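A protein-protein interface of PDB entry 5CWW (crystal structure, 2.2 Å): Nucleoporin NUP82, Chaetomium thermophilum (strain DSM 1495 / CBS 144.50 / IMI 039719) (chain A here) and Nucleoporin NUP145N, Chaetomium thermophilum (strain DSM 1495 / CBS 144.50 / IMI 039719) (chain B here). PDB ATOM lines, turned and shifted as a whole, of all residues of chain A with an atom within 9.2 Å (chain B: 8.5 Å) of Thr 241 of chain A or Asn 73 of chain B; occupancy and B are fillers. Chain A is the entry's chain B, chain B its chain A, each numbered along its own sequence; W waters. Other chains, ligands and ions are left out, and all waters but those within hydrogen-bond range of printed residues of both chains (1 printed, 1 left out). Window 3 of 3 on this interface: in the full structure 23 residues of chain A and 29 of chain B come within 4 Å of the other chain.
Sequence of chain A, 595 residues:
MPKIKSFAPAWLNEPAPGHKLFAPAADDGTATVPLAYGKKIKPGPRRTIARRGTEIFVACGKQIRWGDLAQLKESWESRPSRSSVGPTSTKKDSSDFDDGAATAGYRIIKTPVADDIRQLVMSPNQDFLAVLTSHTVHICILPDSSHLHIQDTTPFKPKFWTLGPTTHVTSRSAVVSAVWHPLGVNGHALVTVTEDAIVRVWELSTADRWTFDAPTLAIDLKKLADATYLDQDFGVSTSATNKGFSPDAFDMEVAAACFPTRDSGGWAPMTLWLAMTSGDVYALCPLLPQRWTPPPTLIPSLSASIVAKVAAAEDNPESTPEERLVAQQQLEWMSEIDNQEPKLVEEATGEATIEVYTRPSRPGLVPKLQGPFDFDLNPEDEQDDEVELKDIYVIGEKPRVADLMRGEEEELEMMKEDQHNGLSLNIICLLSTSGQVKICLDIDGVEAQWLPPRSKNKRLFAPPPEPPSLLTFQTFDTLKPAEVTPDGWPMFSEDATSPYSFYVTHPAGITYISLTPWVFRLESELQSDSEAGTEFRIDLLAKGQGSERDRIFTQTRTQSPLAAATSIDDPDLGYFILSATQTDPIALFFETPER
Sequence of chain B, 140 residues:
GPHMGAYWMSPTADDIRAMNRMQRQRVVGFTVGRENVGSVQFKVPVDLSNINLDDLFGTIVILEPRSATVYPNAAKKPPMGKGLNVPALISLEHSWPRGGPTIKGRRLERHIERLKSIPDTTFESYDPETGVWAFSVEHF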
ATOM      1  N   THR A 166      15.002  -0.456  10.398  1.00  0.00           N
ATOM      2  CA  THR A 166      13.700   0.036  10.850  1.00  0.00           C
ATOM      3  C   THR A 166      13.387  -0.439  12.268  1.00  0.00           C
ATOM      4  O   THR A 166      12.318  -0.144  12.806  1.00  0.00           O
ATOM      5  CB  THR A 166      12.564  -0.416   9.904  1.00  0.00           C
ATOM      6  OG1 THR A 166      12.362  -1.830  10.024  1.00  0.00           O
ATOM      7  CG2 THR A 166      12.896  -0.071   8.459  1.00  0.00           C
ATOM      8  N   THR A 167      14.326  -1.169  12.865  1.00  0.00           N
ATOM      9  CA  THR A 167      14.136  -1.772  14.181  1.00  0.00           C
ATOM     10  C   THR A 167      14.964  -1.047  15.241  1.00  0.00           C
ATOM     11  O   THR A 167      14.421  -0.470  16.182  1.00  0.00           O
ATOM     12  CB  THR A 167      14.521  -3.264  14.164  1.00  0.00           C
ATOM     13  OG1 THR A 167      13.801  -3.930  13.119  1.00  0.00           O
ATOM     14  CG2 THR A 167      14.199  -3.920  15.496  1.00  0.00           C
ATOM     15  N   VAL A 169      16.519   1.904  15.955  1.00  0.00           N
ATOM     16  CA  VAL A 169      16.498   3.286  15.492  1.00  0.00           C
ATOM     17  C   VAL A 169      16.236   4.210  16.677  1.00  0.00           C
ATOM     18  O   VAL A 169      15.709   3.779  17.704  1.00  0.00           O
ATOM     19  CB  VAL A 169      15.410   3.498  14.413  1.00  0.00           C
ATOM     20  CG1 VAL A 169      15.582   4.837  13.713  1.00  0.00           C
ATOM     21  CG2 VAL A 169      15.459   2.381  13.389  1.00  0.00           C
ATOM     22  N   SER A 171      14.056   6.341  17.021  1.00  0.00           N
ATOM     23  CA  SER A 171      12.625   6.535  17.241  1.00  0.00           C
ATOM     24  C   SER A 171      11.994   5.345  17.963  1.00  0.00           C
ATOM     25  O   SER A 171      10.805   5.375  18.281  1.00  0.00           O
ATOM     26  CB  SER A 171      11.903   6.782  15.910  1.00  0.00           C
ATOM     27  OG  SER A 171      12.048   5.688  15.022  1.00  0.00           O
ATOM     28  N   ARG A 172      12.785   4.302  18.217  1.00  0.00           N
ATOM     29  CA  ARG A 172      12.301   3.118  18.922  1.00  0.00           C
ATOM     30  C   ARG A 172      13.089   2.907  20.211  1.00  0.00           C
ATOM     31  O   ARG A 172      13.869   3.768  20.614  1.00  0.00           O
ATOM     32  CB  ARG A 172      12.409   1.878  18.028  1.00  0.00           C
ATOM     33  CG  ARG A 172      11.504   1.905  16.806  1.00  0.00           C
ATOM     34  CD  ARG A 172      10.049   1.624  17.164  1.00  0.00           C
ATOM     35  NE  ARG A 172       9.482   0.566  16.330  1.00  0.00           N
ATOM     36  CZ  ARG A 172       9.278  -0.693  16.716  1.00  0.00           C
ATOM     37  NH1 ARG A 172       9.577  -1.089  17.946  1.00  0.00           N
ATOM     38  NH2 ARG A 172       8.760  -1.564  15.861  1.00  0.00           N
ATOM     39  N   SER A 173      12.883   1.764  20.858  1.00  0.00           N
ATOM     40  CA  SER A 173      13.518   1.486  22.142  1.00  0.00           C
ATOM     41  C   SER A 173      15.032   1.342  22.007  1.00  0.00           C
ATOM     42  O   SER A 173      15.528   0.746  21.051  1.00  0.00           O
ATOM     43  CB  SER A 173      12.929   0.219  22.760  1.00  0.00           C
ATOM     44  OG  SER A 173      13.476  -0.023  24.045  1.00  0.00           O
ATOM     45  N   ASP A 196      12.976  -2.157  26.346  1.00  0.00           N
ATOM     46  CA  ASP A 196      11.592  -2.605  26.478  1.00  0.00           C
ATOM     47  C   ASP A 196      11.493  -4.121  26.305  1.00  0.00           C
ATOM     48  O   ASP A 196      10.445  -4.651  25.940  1.00  0.00           O
ATOM     49  CB  ASP A 196      10.686  -1.874  25.476  1.00  0.00           C
ATOM     50  CG  ASP A 196      11.035  -2.169  24.028  1.00  0.00           C
ATOM     51  OD1 ASP A 196      12.176  -2.591  23.750  1.00  0.00           O
ATOM     52  OD2 ASP A 196      10.159  -1.963  23.162  1.00  0.00           O
ATOM     53  N   VAL A 236       6.618  -9.412  17.384  1.00  0.00           N
ATOM     54  CA  VAL A 236       6.602  -7.958  17.372  1.00  0.00           C
ATOM     55  C   VAL A 236       6.052  -7.462  16.042  1.00  0.00           C
ATOM     56  O   VAL A 236       6.354  -8.019  14.985  1.00  0.00           O
ATOM     57  CB  VAL A 236       8.009  -7.371  17.599  1.00  0.00           C
ATOM     58  CG1 VAL A 236       7.957  -5.851  17.632  1.00  0.00           C
ATOM     59  CG2 VAL A 236       8.605  -7.905  18.892  1.00  0.00           C
ATOM     60  N   SER A 237       5.244  -6.413  16.107  1.00  0.00           N
ATOM     61  CA  SER A 237       4.650  -5.825  14.919  1.00  0.00           C
ATOM     62  C   SER A 237       5.486  -4.664  14.412  1.00  0.00           C
ATOM     63  O   SER A 237       5.870  -3.781  15.177  1.00  0.00           O
ATOM     64  CB  SER A 237       3.231  -5.348  15.209  1.00  0.00           C
ATOM     65  OG  SER A 237       2.715  -4.641  14.096  1.00  0.00           O
ATOM     66  N   THR A 238       5.754  -4.670  13.112  1.00  0.00           N
ATOM     67  CA  THR A 238       6.460  -3.574  12.471  1.00  0.00           C
ATOM     68  C   THR A 238       5.649  -2.286  12.585  1.00  0.00           C
ATOM     69  O   THR A 238       6.213  -1.198  12.693  1.00  0.00           O
ATOM     70  CB  THR A 238       6.742  -3.891  10.987  1.00  0.00           C
ATOM     71  OG1 THR A 238       7.595  -5.040  10.902  1.00  0.00           O
ATOM     72  CG2 THR A 238       7.414  -2.715  10.285  1.00  0.00           C
ATOM     73  N   SER A 239       4.326  -2.423  12.577  1.00  0.00           N
ATOM     74  CA  SER A 239       3.428  -1.273  12.633  1.00  0.00           C
ATOM     75  C   SER A 239       3.303  -0.675  14.033  1.00  0.00           C
ATOM     76  O   SER A 239       2.939   0.491  14.183  1.00  0.00           O
ATOM     77  CB  SER A 239       2.040  -1.673  12.132  1.00  0.00           C
ATOM     78  OG  SER A 239       2.110  -2.224  10.830  1.00  0.00           O
ATOM     79  N   ALA A 240       3.599  -1.469  15.056  1.00  0.00           N
ATOM     80  CA  ALA A 240       3.468  -1.014  16.438  1.00  0.00           C
ATOM     81  C   ALA A 240       4.596  -0.065  16.821  1.00  0.00           C
ATOM     82  O   ALA A 240       5.566  -0.469  17.459  1.00  0.00           O
ATOM     83  CB  ALA A 240       3.437  -2.206  17.380  1.00  0.00           C
ATOM     84  N   THR A 241       4.459   1.198  16.432  1.00  0.00           N
ATOM     85  CA  THR A 241       5.504   2.199  16.645  1.00  0.00           C
ATOM     86  C   THR A 241       5.185   3.151  17.801  1.00  0.00           C
ATOM     87  O   THR A 241       6.091   3.712  18.412  1.00  0.00           O
ATOM     88  CB  THR A 241       5.734   3.033  15.374  1.00  0.00           C
ATOM     89  OG1 THR A 241       4.482   3.552  14.907  1.00  0.00           O
ATOM     90  CG2 THR A 241       6.362   2.178  14.285  1.00  0.00           C
ATOM     91  N   ASN A 242       3.899   3.336  18.088  1.00  0.00           N
ATOM     92  CA  ASN A 242       3.477   4.194  19.191  1.00  0.00           C
ATOM     93  C   ASN A 242       3.434   3.414  20.500  1.00  0.00           C
ATOM     94  O   ASN A 242       2.772   2.379  20.593  1.00  0.00           O
ATOM     95  CB  ASN A 242       2.106   4.809  18.898  1.00  0.00           C
ATOM     96  CG  ASN A 242       1.715   5.878  19.905  1.00  0.00           C
ATOM     97  OD1 ASN A 242       2.570   6.560  20.470  1.00  0.00           O
ATOM     98  ND2 ASN A 242       0.419   6.029  20.131  1.00  0.00           N
ATOM     99  N   LYS A 243       4.143   3.910  21.508  1.00  0.00           N
ATOM    100  CA  LYS A 243       4.218   3.225  22.793  1.00  0.00           C
ATOM    101  C   LYS A 243       2.937   3.411  23.598  1.00  0.00           C
ATOM    102  O   LYS A 243       2.346   4.491  23.605  1.00  0.00           O
ATOM    103  CB  LYS A 243       5.417   3.733  23.596  1.00  0.00           C
ATOM    104  CG  LYS A 243       6.758   3.518  22.910  1.00  0.00           C
ATOM    105  CD  LYS A 243       7.370   4.836  22.452  1.00  0.00           C
ATOM    106  CE  LYS A 243       8.718   4.622  21.775  1.00  0.00           C
ATOM    107  NZ  LYS A 243       8.597   3.817  20.527  1.00  0.00           N
ATOM    108  N   GLY A 244       2.514   2.344  24.268  1.00  0.00           N
ATOM    109  CA  GLY A 244       1.372   2.395  25.162  1.00  0.00           C
ATOM    110  C   GLY A 244       1.803   2.662  26.593  1.00  0.00           C
ATOM    111  O   GLY A 244       2.846   3.273  26.835  1.00  0.00           O
ATOM    112  N   THR B  59      -7.517  -2.816  17.307  1.00  0.00           N
ATOM    113  CA  THR B  59      -6.985  -2.056  16.179  1.00  0.00           C
ATOM    114  C   THR B  59      -6.597  -0.642  16.601  1.00  0.00           C
ATOM    115  O   THR B  59      -5.473  -0.204  16.361  1.00  0.00           O
ATOM    116  CB  THR B  59      -8.002  -1.985  15.030  1.00  0.00           C
ATOM    117  OG1 THR B  59      -8.339  -3.314  14.612  1.00  0.00           O
ATOM    118  CG2 THR B  59      -7.434  -1.212  13.844  1.00  0.00           C
ATOM    119  N   ILE B  60      -7.535   0.067  17.220  1.00  0.00           N
ATOM    120  CA  ILE B  60      -7.283   1.419  17.707  1.00  0.00           C
ATOM    121  C   ILE B  60      -6.980   1.387  19.202  1.00  0.00           C
ATOM    122  O   ILE B  60      -6.044   2.032  19.666  1.00  0.00           O
ATOM    123  CB  ILE B  60      -8.478   2.350  17.440  1.00  0.00           C
ATOM    124  CG1 ILE B  60      -8.773   2.407  15.937  1.00  0.00           C
ATOM    125  CG2 ILE B  60      -8.195   3.750  17.973  1.00  0.00           C
ATOM    126  CD1 ILE B  60     -10.079   3.100  15.579  1.00  0.00           C
ATOM    127  N   ILE B  62      -5.944  -1.143  22.158  1.00  0.00           N
ATOM    128  CA  ILE B  62      -5.419  -2.461  22.486  1.00  0.00           C
ATOM    129  C   ILE B  62      -5.257  -2.588  23.990  1.00  0.00           C
ATOM    130  O   ILE B  62      -4.468  -1.868  24.604  1.00  0.00           O
ATOM    131  CB  ILE B  62      -4.068  -2.724  21.797  1.00  0.00           C
ATOM    132  CG1 ILE B  62      -4.241  -2.677  20.276  1.00  0.00           C
ATOM    133  CG2 ILE B  62      -3.505  -4.077  22.227  1.00  0.00           C
ATOM    134  CD1 ILE B  62      -2.947  -2.806  19.493  1.00  0.00           C
ATOM    135  N   THR B  69      -2.873   0.525  25.059  1.00  0.00           N
ATOM    136  CA  THR B  69      -2.366   1.295  23.929  1.00  0.00           C
ATOM    137  C   THR B  69      -3.512   1.835  23.074  1.00  0.00           C
ATOM    138  O   THR B  69      -4.392   1.081  22.657  1.00  0.00           O
ATOM    139  CB  THR B  69      -1.435   0.439  23.047  1.00  0.00           C
ATOM    140  OG1 THR B  69      -0.485  -0.246  23.873  1.00  0.00           O
ATOM    141  CG2 THR B  69      -0.697   1.304  22.036  1.00  0.00           C
ATOM    142  N   VAL B  70      -3.496   3.143  22.828  1.00  0.00           N
ATOM    143  CA  VAL B  70      -4.441   3.777  21.912  1.00  0.00           C
ATOM    144  C   VAL B  70      -3.682   4.339  20.713  1.00  0.00           C
ATOM    145  O   VAL B  70      -2.702   5.065  20.875  1.00  0.00           O
ATOM    146  CB  VAL B  70      -5.242   4.900  22.596  1.00  0.00           C
ATOM    147  CG1 VAL B  70      -6.309   5.442  21.653  1.00  0.00           C
ATOM    148  CG2 VAL B  70      -5.884   4.392  23.878  1.00  0.00           C
ATOM    149  N   TYR B  71      -4.154   4.002  19.514  1.00  0.00           N
ATOM    150  CA  TYR B  71      -3.442   4.300  18.272  1.00  0.00           C
ATOM    151  C   TYR B  71      -2.024   3.728  18.319  1.00  0.00           C
ATOM    152  O   TYR B  71      -1.057   4.471  18.481  1.00  0.00           O
ATOM    153  CB  TYR B  71      -3.398   5.808  18.009  1.00  0.00           C
ATOM    154  CG  TYR B  71      -4.759   6.440  17.810  1.00  0.00           C
ATOM    155  CD1 TYR B  71      -5.553   6.101  16.723  1.00  0.00           C
ATOM    156  CD2 TYR B  71      -5.243   7.382  18.706  1.00  0.00           C
ATOM    157  CE1 TYR B  71      -6.800   6.677  16.539  1.00  0.00           C
ATOM    158  CE2 TYR B  71      -6.483   7.964  18.532  1.00  0.00           C
ATOM    159  CZ  TYR B  71      -7.258   7.609  17.448  1.00  0.00           C
ATOM    160  OH  TYR B  71      -8.492   8.191  17.275  1.00  0.00           O
ATOM    161  N   PRO B  72      -1.899   2.398  18.172  1.00  0.00           N
ATOM    162  CA  PRO B  72      -0.599   1.722  18.260  1.00  0.00           C
ATOM    163  C   PRO B  72       0.332   2.081  17.105  1.00  0.00           C
ATOM    164  O   PRO B  72       1.553   2.078  17.275  1.00  0.00           O
ATOM    165  CB  PRO B  72      -0.972   0.236  18.225  1.00  0.00           C
ATOM    166  CG  PRO B  72      -2.277   0.191  17.527  1.00  0.00           C
ATOM    167  CD  PRO B  72      -2.994   1.446  17.918  1.00  0.00           C
ATOM    168  N   ASN B  73      -0.244   2.377  15.945  1.00  0.00           N
ATOM    169  CA  ASN B  73       0.522   2.853  14.802  1.00  0.00           C
ATOM    170  C   ASN B  73       0.686   4.368  14.878  1.00  0.00           C
ATOM    171  O   ASN B  73      -0.278   5.112  14.709  1.00  0.00           O
ATOM    172  CB  ASN B  73      -0.167   2.458  13.494  1.00  0.00           C
ATOM    173  CG  ASN B  73       0.730   2.622  12.283  1.00  0.00           C
ATOM    174  OD1 ASN B  73       1.563   3.526  12.226  1.00  0.00           O
ATOM    175  ND2 ASN B  73       0.552   1.751  11.297  1.00  0.00           N
ATOM    176  N   ALA B  74       1.910   4.815  15.139  1.00  0.00           N
ATOM    177  CA  ALA B  74       2.182   6.234  15.334  1.00  0.00           C
ATOM    178  C   ALA B  74       1.886   7.044  14.075  1.00  0.00           C
ATOM    179  O   ALA B  74       1.488   8.206  14.156  1.00  0.00           O
ATOM    180  CB  ALA B  74       3.629   6.438  15.761  1.00  0.00           C
ATOM    181  N   ALA B  75       2.077   6.424  12.916  1.00  0.00           N
ATOM    182  CA  ALA B  75       1.884   7.108  11.641  1.00  0.00           C
ATOM    183  C   ALA B  75       0.413   7.416  11.380  1.00  0.00           C
ATOM    184  O   ALA B  75       0.087   8.437  10.774  1.00  0.00           O
ATOM    185  CB  ALA B  75       2.453   6.271  10.506  1.00  0.00           C
ATOM    186  N   LYS B  76      -0.469   6.534  11.843  1.00  0.00           N
ATOM    187  CA  LYS B  76      -1.903   6.680  11.612  1.00  0.00           C
ATOM    188  C   LYS B  76      -2.628   7.244  12.833  1.00  0.00           C
ATOM    189  O   LYS B  76      -3.844   7.101  12.965  1.00  0.00           O
ATOM    190  CB  LYS B  76      -2.509   5.332  11.212  1.00  0.00           C
ATOM    191  CG  LYS B  76      -1.907   4.754   9.937  1.00  0.00           C
ATOM    192  CD  LYS B  76      -2.615   3.484   9.493  1.00  0.00           C
ATOM    193  CE  LYS B  76      -2.005   2.933   8.212  1.00  0.00           C
ATOM    194  NZ  LYS B  76      -2.722   1.725   7.715  1.00  0.00           N
ATOM    195  N   LYS B  77      -1.878   7.896  13.716  1.00  0.00           N
ATOM    196  CA  LYS B  77      -2.455   8.521  14.904  1.00  0.00           C
ATOM    197  C   LYS B  77      -2.947   9.933  14.581  1.00  0.00           C
ATOM    198  O   LYS B  77      -2.199  10.727  14.019  1.00  0.00           O
ATOM    199  CB  LYS B  77      -1.424   8.570  16.034  1.00  0.00           C
ATOM    200  CG  LYS B  77      -1.923   9.256  17.301  1.00  0.00           C
ATOM    201  CD  LYS B  77      -0.940   9.095  18.452  1.00  0.00           C
ATOM    202  CE  LYS B  77       0.376   9.809  18.182  1.00  0.00           C
ATOM    203  NZ  LYS B  77       1.332   9.659  19.314  1.00  0.00           N
ATOM    204  N   PRO B  78      -4.206  10.255  14.929  1.00  0.00           N
ATOM    205  CA  PRO B  78      -4.700  11.603  14.617  1.00  0.00           C
ATOM    206  C   PRO B  78      -3.983  12.690  15.413  1.00  0.00           C
ATOM    207  O   PRO B  78      -3.308  12.376  16.392  1.00  0.00           O
ATOM    208  CB  PRO B  78      -6.182  11.544  15.012  1.00  0.00           C
ATOM    209  CG  PRO B  78      -6.507  10.097  15.143  1.00  0.00           C
ATOM    210  CD  PRO B  78      -5.245   9.429  15.566  1.00  0.00           C
ATOM    211  N   PHE B 140      -2.114  10.523  23.528  1.00  0.00           N
ATOM    212  CA  PHE B 140      -1.449   9.253  23.250  1.00  0.00           C
ATOM    213  C   PHE B 140      -0.361   9.431  22.194  1.00  0.00           C
ATOM    214  O   PHE B 140       0.070   8.474  21.548  1.00  0.00           O
ATOM    215  CB  PHE B 140      -2.468   8.210  22.794  1.00  0.00           C
ATOM    216  CG  PHE B 140      -3.470   7.846  23.852  1.00  0.00           C
ATOM    217  CD1 PHE B 140      -3.183   6.869  24.792  1.00  0.00           C
ATOM    218  CD2 PHE B 140      -4.703   8.480  23.903  1.00  0.00           C
ATOM    219  CE1 PHE B 140      -4.105   6.533  25.767  1.00  0.00           C
ATOM    220  CE2 PHE B 140      -5.628   8.146  24.875  1.00  0.00           C
ATOM    221  CZ  PHE B 140      -5.329   7.172  25.809  1.00  0.00           C
ATOM    222  OXT PHE B 140       0.116  10.542  21.961  1.00  0.00           O
HETATM  223  O   HOH W   1      -0.823   4.585  23.134  1.00  0.00           O
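Of the printed residues of chain B, Ser 239 of chain A touches Pro 72 and Asn 73. Thr 241 of chain A touches just these residues of chain B: Pro 72 (3.2 Å), Asn 73 (3.9 Å) and Ala 74 (2.9 Å). Pro 72 of chain B touches four residues of chain A. Of chain A, only Thr 241 and Asn 242 come within 4 Å of Ala 74 of chain B. Printed residues of chain A within 4 Å of Lys 77 of chain B: Asn 242. The nearest residue of chain B that does not touch Thr 241 of chain A is Ala 75 of chain B (4.2 Å). The nearest residue of chain A that does not touch Asn 73 of chain B is Asn 242 of chain A (4.3 Å).
The backbone NH (N) of Ala 74 of chain B is in hydrogen-bond range of the side-chain hydroxyl (OG1) of Thr 241 of chain A (2.9 Å). N of Thr 241 of chain A lies within hydrogen-bond range of O of Pro 72 of chain B, at 3.2 Å. O of Pro 72 of chain B is in hydrogen-bond range of N of Asn 242 of chain A (2.8 Å). The chain-end carboxylate (O) of Phe 140 of chain B is in hydrogen-bond range of the side-chain amide nitrogen (ND2) of Asn 242 of chain A (2.8 Å). The backbone carbonyl oxygen (O) of Val 70 of chain B sits at hydrogen-bond distance from the side-chain amide nitrogen (ND2) of Asn 242 of chain A (3.4 Å). O of Tyr 71 of chain B sits at hydrogen-bond distance from ND2 of Asn 242 of chain A, at 2.7 Å.
The side-chain amino group of Lys 77 of chain B lies within salt-bridge range of the chain-end carboxylate of Phe 140 of chain B (2.8 Å). The backbone NH of Ser 239 of chain A lies close to the side-chain hydroxyl of Ser 237 of chain A (3.1 Å). OD1 of Asn 73 of chain B is in hydrogen-bond range of N of Ala 75 of chain B (3.0 Å). N of Ala 240 of chain A sits at hydrogen-bond distance from OG of Ser 237 of chain A (3.4 Å). O of Thr 69 of chain B sits at hydrogen-bond distance from N of Ile 62 of chain B, at 2.8 Å. The backbone carbonyl oxygen of Thr 241 of chain A lies within hydrogen-bond range of the side-chain amino group of Lys 243 of chain A, at 3.3 Å.
Among the printed residues, merely in contact across the chains: Ser 239 of chain A with Pro 72 of chain B (3.7 Å), Ser 239 of chain A with Asn 73 of chain B (3.4 Å), Ala 240 of chain A with Pro 72 of chain B (3.7 Å), Thr 241 of chain A with Asn 73 of chain B (3.9 Å), Asn 242 of chain A with Thr 69 of chain B (3.9 Å), Asn 242 of chain A with Ala 74 of chain B (3.8 Å), Asn 242 of chain A with Lys 77 of chain B (3.5 Å) and Gly 244 of chain A with Thr 69 of chain B (3.5 Å).
Hydrophobic or aromatic side chains of chain B that line the printed part of chain A: Ala 74. Printed residues of chain A that touch a printed residue of chain B: Ser 239, Ala 240, Thr 241, Asn 242 and Gly 244. Among the printed residues, 14 pairs touch across the chains. Among the printed residues, no Asp or Glu carboxylate lies within 4 Å of a Lys or Arg side-chain nitrogen of the other chain.
Water W1 lies within hydrogen-bond range of the backbone carbonyl oxygen (O) of Val 70 of chain B (3.0 Å) and the backbone carbonyl oxygen (O) of Lys 243 of chain A (3.2 Å).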
